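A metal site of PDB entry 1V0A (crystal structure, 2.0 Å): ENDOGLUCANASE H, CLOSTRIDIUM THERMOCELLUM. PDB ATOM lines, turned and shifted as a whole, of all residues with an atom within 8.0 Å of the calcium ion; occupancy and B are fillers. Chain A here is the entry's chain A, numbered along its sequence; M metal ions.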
ATOM      1  N   GLU A  91     -10.763  -6.286  -1.541  1.00  0.00           N
ATOM      2  CA  GLU A  91      -9.699  -6.173  -0.554  1.00  0.00           C
ATOM      3  C   GLU A  91      -8.544  -5.334  -1.117  1.00  0.00           C
ATOM      4  O   GLU A  91      -8.543  -5.003  -2.296  1.00  0.00           O
ATOM      5  CB  GLU A  91      -9.184  -7.553  -0.164  1.00  0.00           C
ATOM      6  CG  GLU A  91     -10.123  -8.347   0.729  1.00  0.00           C
ATOM      7  CD  GLU A  91      -9.710  -9.804   0.844  1.00  0.00           C
ATOM      8  OE1 GLU A  91      -8.568 -10.151   0.479  1.00  0.00           O
ATOM      9  OE2 GLU A  91     -10.541 -10.620   1.307  1.00  0.00           O
ATOM     10  N   LYS A  92      -7.587  -4.995  -0.254  1.00  0.00           N
ATOM     11  CA  LYS A  92      -6.374  -4.314  -0.690  1.00  0.00           C
ATOM     12  C   LYS A  92      -5.433  -5.317  -1.360  1.00  0.00           C
ATOM     13  O   LYS A  92      -5.396  -6.489  -0.991  1.00  0.00           O
ATOM     14  CB  LYS A  92      -5.670  -3.658   0.503  1.00  0.00           C
ATOM     15  CG  LYS A  92      -6.440  -2.500   1.133  1.00  0.00           C
ATOM     16  CD  LYS A  92      -5.544  -1.721   2.080  1.00  0.00           C
ATOM     17  CE  LYS A  92      -6.303  -1.272   3.322  1.00  0.00           C
ATOM     18  NZ  LYS A  92      -5.481  -0.351   4.163  1.00  0.00           N
ATOM     19  N   ILE A  94      -2.045  -7.337  -2.457  1.00  0.00           N
ATOM     20  CA  ILE A  94      -0.896  -7.892  -1.734  1.00  0.00           C
ATOM     21  C   ILE A  94       0.400  -7.142  -2.073  1.00  0.00           C
ATOM     22  O   ILE A  94       1.381  -7.239  -1.336  1.00  0.00           O
ATOM     23  CB  ILE A  94      -0.713  -9.415  -2.015  1.00  0.00           C
ATOM     24  CG1 ILE A  94      -0.741  -9.707  -3.518  1.00  0.00           C
ATOM     25  CG2 ILE A  94      -1.762 -10.208  -1.266  1.00  0.00           C
ATOM     26  CD1 ILE A  94       0.321 -10.701  -3.965  1.00  0.00           C
ATOM     27  N   GLY A 100      -7.373  -5.970  -4.386  1.00  0.00           N
ATOM     28  CA  GLY A 100      -7.122  -7.373  -4.085  1.00  0.00           C
ATOM     29  C   GLY A 100      -8.366  -8.203  -4.322  1.00  0.00           C
ATOM     30  O   GLY A 100      -9.200  -7.845  -5.156  1.00  0.00           O
ATOM     31  N   GLU A 101      -8.489  -9.304  -3.580  1.00  0.00           N
ATOM     32  CA  GLU A 101      -9.573 -10.267  -3.756  1.00  0.00           C
ATOM     33  C   GLU A 101     -10.948  -9.606  -3.869  1.00  0.00           C
ATOM     34  O   GLU A 101     -11.324  -8.799  -3.017  1.00  0.00           O
ATOM     35  CB  GLU A 101      -9.560 -11.289  -2.612  1.00  0.00           C
ATOM     36  CG  GLU A 101     -10.110 -12.659  -2.972  1.00  0.00           C
ATOM     37  CD  GLU A 101      -9.821 -13.699  -1.908  1.00  0.00           C
ATOM     38  OE1 GLU A 101      -9.953 -13.370  -0.713  1.00  0.00           O
ATOM     39  OE2 GLU A 101      -9.479 -14.839  -2.272  1.00  0.00           O
ATOM     40  N   HIS A 102     -11.682  -9.967  -4.924  1.00  0.00           N
ATOM     41  CA  HIS A 102     -13.031  -9.468  -5.151  1.00  0.00           C
ATOM     42  C   HIS A 102     -14.063 -10.384  -4.497  1.00  0.00           C
ATOM     43  O   HIS A 102     -13.977 -11.605  -4.615  1.00  0.00           O
ATOM     44  CB  HIS A 102     -13.319  -9.362  -6.657  1.00  0.00           C
ATOM     45  CG  HIS A 102     -12.664  -8.185  -7.332  1.00  0.00           C
ATOM     46  ND1 HIS A 102     -12.929  -7.836  -8.631  1.00  0.00           N
ATOM     47  CD2 HIS A 102     -11.749  -7.291  -6.877  1.00  0.00           C
ATOM     48  CE1 HIS A 102     -12.207  -6.781  -8.967  1.00  0.00           C
ATOM     49  NE2 HIS A 102     -11.484  -6.437  -7.913  1.00  0.00           N
ATOM     50  N   TRP A 103     -15.035  -9.768  -3.830  1.00  0.00           N
ATOM     51  CA  TRP A 103     -16.120 -10.493  -3.171  1.00  0.00           C
ATOM     52  C   TRP A 103     -17.466  -9.907  -3.609  1.00  0.00           C
ATOM     53  O   TRP A 103     -17.658  -8.694  -3.551  1.00  0.00           O
ATOM     54  CB  TRP A 103     -15.942 -10.457  -1.657  1.00  0.00           C
ATOM     55  CG  TRP A 103     -14.826 -11.348  -1.216  1.00  0.00           C
ATOM     56  CD1 TRP A 103     -13.484 -11.055  -1.206  1.00  0.00           C
ATOM     57  CD2 TRP A 103     -14.929 -12.701  -0.763  1.00  0.00           C
ATOM     58  NE1 TRP A 103     -12.766 -12.130  -0.761  1.00  0.00           N
ATOM     59  CE2 TRP A 103     -13.624 -13.163  -0.479  1.00  0.00           C
ATOM     60  CE3 TRP A 103     -16.000 -13.576  -0.551  1.00  0.00           C
ATOM     61  CZ2 TRP A 103     -13.359 -14.447  -0.007  1.00  0.00           C
ATOM     62  CZ3 TRP A 103     -15.746 -14.863  -0.086  1.00  0.00           C
ATOM     63  CH2 TRP A 103     -14.438 -15.278   0.182  1.00  0.00           C
ATOM     64  N   ARG A 125     -16.838 -15.395  -3.183  1.00  0.00           N
ATOM     65  CA  ARG A 125     -15.588 -15.098  -3.896  1.00  0.00           C
ATOM     66  C   ARG A 125     -15.820 -15.075  -5.408  1.00  0.00           C
ATOM     67  O   ARG A 125     -16.328 -16.035  -5.984  1.00  0.00           O
ATOM     68  CB  ARG A 125     -14.505 -16.106  -3.525  1.00  0.00           C
ATOM     69  CG  ARG A 125     -13.102 -15.683  -3.944  1.00  0.00           C
ATOM     70  CD  ARG A 125     -12.001 -16.626  -3.495  1.00  0.00           C
ATOM     71  NE  ARG A 125     -10.755 -16.361  -4.211  1.00  0.00           N
ATOM     72  CZ  ARG A 125     -10.382 -16.975  -5.332  1.00  0.00           C
ATOM     73  NH1 ARG A 125     -11.156 -17.906  -5.877  1.00  0.00           N
ATOM     74  NH2 ARG A 125      -9.230 -16.662  -5.902  1.00  0.00           N
ATOM     75  N   GLN A 134      -4.717  -9.989  -5.939  1.00  0.00           N
ATOM     76  CA  GLN A 134      -5.544 -10.776  -5.008  1.00  0.00           C
ATOM     77  C   GLN A 134      -4.696 -11.710  -4.138  1.00  0.00           C
ATOM     78  O   GLN A 134      -3.654 -12.199  -4.572  1.00  0.00           O
ATOM     79  CB  GLN A 134      -6.616 -11.563  -5.770  1.00  0.00           C
ATOM     80  CG  GLN A 134      -6.090 -12.694  -6.662  1.00  0.00           C
ATOM     81  CD  GLN A 134      -6.945 -13.948  -6.615  1.00  0.00           C
ATOM     82  OE1 GLN A 134      -7.653 -14.193  -5.639  1.00  0.00           O
ATOM     83  NE2 GLN A 134      -6.891 -14.754  -7.672  1.00  0.00           N
ATOM     84  N   ASP A 135      -5.150 -11.940  -2.909  1.00  0.00           N
ATOM     85  CA  ASP A 135      -4.390 -12.775  -1.959  1.00  0.00           C
ATOM     86  C   ASP A 135      -4.674 -14.270  -2.070  1.00  0.00           C
ATOM     87  O   ASP A 135      -3.965 -15.078  -1.463  1.00  0.00           O
ATOM     88  CB  ASP A 135      -4.569 -12.282  -0.513  1.00  0.00           C
ATOM     89  CG  ASP A 135      -5.984 -12.454   0.009  1.00  0.00           C
ATOM     90  OD1 ASP A 135      -6.893 -12.857  -0.757  1.00  0.00           O
ATOM     91  OD2 ASP A 135      -6.293 -12.200   1.197  1.00  0.00           O
ATOM     92  N   MET A 136      -5.691 -14.625  -2.853  1.00  0.00           N
ATOM     93  CA  MET A 136      -6.094 -16.021  -3.060  1.00  0.00           C
ATOM     94  C   MET A 136      -6.396 -16.767  -1.744  1.00  0.00           C
ATOM     95  O   MET A 136      -6.244 -17.989  -1.673  1.00  0.00           O
ATOM     96  CB  MET A 136      -5.023 -16.788  -3.843  1.00  0.00           C
ATOM     97  CG  MET A 136      -4.970 -16.499  -5.329  1.00  0.00           C
ATOM     98  SD  MET A 136      -3.563 -17.525  -6.211  1.00  0.00           S
ATOM     99  CE  MET A 136      -2.009 -16.501  -5.595  1.00  0.00           C
ATOM    100  N   SER A 137      -6.819 -16.028  -0.720  1.00  0.00           N
ATOM    101  CA  SER A 137      -7.023 -16.611   0.604  1.00  0.00           C
ATOM    102  C   SER A 137      -8.352 -17.335   0.754  1.00  0.00           C
ATOM    103  O   SER A 137      -8.496 -18.215   1.603  1.00  0.00           O
ATOM    104  CB  SER A 137      -6.842 -15.556   1.707  1.00  0.00           C
ATOM    105  OG  SER A 137      -7.999 -14.733   1.817  1.00  0.00           O
ATOM    106  N   GLY A 138      -9.342 -16.948  -0.061  1.00  0.00           N
ATOM    107  CA  GLY A 138     -10.663 -17.527   0.014  1.00  0.00           C
ATOM    108  C   GLY A 138     -11.471 -17.067   1.217  1.00  0.00           C
ATOM    109  O   GLY A 138     -12.522 -17.627   1.516  1.00  0.00           O
ATOM    110  N   THR A 139     -10.948 -16.056   1.913  1.00  0.00           N
ATOM    111  CA  THR A 139     -11.645 -15.435   3.044  1.00  0.00           C
ATOM    112  C   THR A 139     -11.722 -13.937   2.832  1.00  0.00           C
ATOM    113  O   THR A 139     -10.731 -13.306   2.437  1.00  0.00           O
ATOM    114  CB  THR A 139     -10.906 -15.726   4.376  1.00  0.00           C
ATOM    115  OG1 THR A 139      -9.520 -15.402   4.252  1.00  0.00           O
ATOM    116  CG2 THR A 139     -10.911 -17.214   4.694  1.00  0.00           C
ATOM    117  N   LEU A 140     -12.898 -13.354   3.070  1.00  0.00           N
ATOM    118  CA  LEU A 140     -13.058 -11.912   3.011  1.00  0.00           C
ATOM    119  C   LEU A 140     -12.442 -11.299   4.260  1.00  0.00           C
ATOM    120  O   LEU A 140     -12.976 -11.429   5.356  1.00  0.00           O
ATOM    121  CB  LEU A 140     -14.539 -11.513   2.857  1.00  0.00           C
ATOM    122  CG  LEU A 140     -14.887 -10.020   2.929  1.00  0.00           C
ATOM    123  CD1 LEU A 140     -14.166  -9.210   1.850  1.00  0.00           C
ATOM    124  CD2 LEU A 140     -16.387  -9.817   2.823  1.00  0.00           C
ATOM    125  N   ASP A 141     -11.297 -10.655   4.073  1.00  0.00           N
ATOM    126  CA  ASP A 141     -10.552 -10.068   5.191  1.00  0.00           C
ATOM    127  C   ASP A 141     -11.025  -8.654   5.473  1.00  0.00           C
ATOM    128  O   ASP A 141     -10.639  -7.696   4.793  1.00  0.00           O
ATOM    129  CB  ASP A 141      -9.052 -10.129   4.922  1.00  0.00           C
ATOM    130  CG  ASP A 141      -8.595 -11.525   4.557  1.00  0.00           C
ATOM    131  OD1 ASP A 141      -8.622 -12.413   5.441  1.00  0.00           O
ATOM    132  OD2 ASP A 141      -8.207 -11.834   3.408  1.00  0.00           O
ATOM    133  N   LEU A 142     -11.874  -8.535   6.494  1.00  0.00           N
ATOM    134  CA  LEU A 142     -12.559  -7.284   6.803  1.00  0.00           C
ATOM    135  C   LEU A 142     -11.650  -6.175   7.313  1.00  0.00           C
ATOM    136  O   LEU A 142     -12.023  -5.005   7.296  1.00  0.00           O
ATOM    137  CB  LEU A 142     -13.706  -7.553   7.784  1.00  0.00           C
ATOM    138  CG  LEU A 142     -14.863  -8.416   7.275  1.00  0.00           C
ATOM    139  CD1 LEU A 142     -15.852  -8.717   8.394  1.00  0.00           C
ATOM    140  CD2 LEU A 142     -15.569  -7.752   6.094  1.00  0.00           C
ATOM    141  N   ASN A 144      -8.952  -5.324   5.866  1.00  0.00           N
ATOM    142  CA  ASN A 144      -8.165  -4.946   4.703  1.00  0.00           C
ATOM    143  C   ASN A 144      -9.011  -4.582   3.485  1.00  0.00           C
ATOM    144  O   ASN A 144      -8.787  -5.089   2.385  1.00  0.00           O
ATOM    145  CB  ASN A 144      -7.186  -6.087   4.356  1.00  0.00           C
ATOM    146  CG  ASN A 144      -5.993  -5.611   3.548  1.00  0.00           C
ATOM    147  OD1 ASN A 144      -5.422  -4.559   3.825  1.00  0.00           O
ATOM    148  ND2 ASN A 144      -5.613  -6.396   2.548  1.00  0.00           N
HETATM  149 CA    CA M   1      -8.801 -12.543   1.183  1.00  0.00          CA
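The side-chain carboxylate (OE1) of Glu 101 sits close to the indole nitrogen (NE1) of Trp 103, 3.1 Å away. OE2 of Glu 101 sits at hydrogen-bond distance from N of Gly 138, at 3.1 Å. The side-chain carboxylate (OE2) of Glu 101 is in salt-bridge range of the guanidinium group (NE) of Arg 125, at 2.8 Å. The indole nitrogen (NE1) of Trp 103 sits close to the side-chain carboxylate (OE2) of Glu 91, 3.4 Å away. The backbone carbonyl oxygen (O) of Glu 91 lies within hydrogen-bond range of the backbone NH (N) of Gly 100.
Of the 18 residues printed, 6 come within 4 Å of the calcium ion. The nearest printed residue that does not touch the calcium ion is Trp 103 (4.4 Å).
The calcium ion is bound by OE1 of Glu 101 (2.4 Å), OD2 of Asp 141 (2.4 Å), OG of Ser 137 (2.4 Å), O of Thr 139 (2.4 Å), OE1 of Glu 91 (2.5 Å), OD2 of Asp 135 (2.5 Å), OE2 of Glu 91 (2.6 Å) and OD1 of Asp 135 (2.7 Å).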
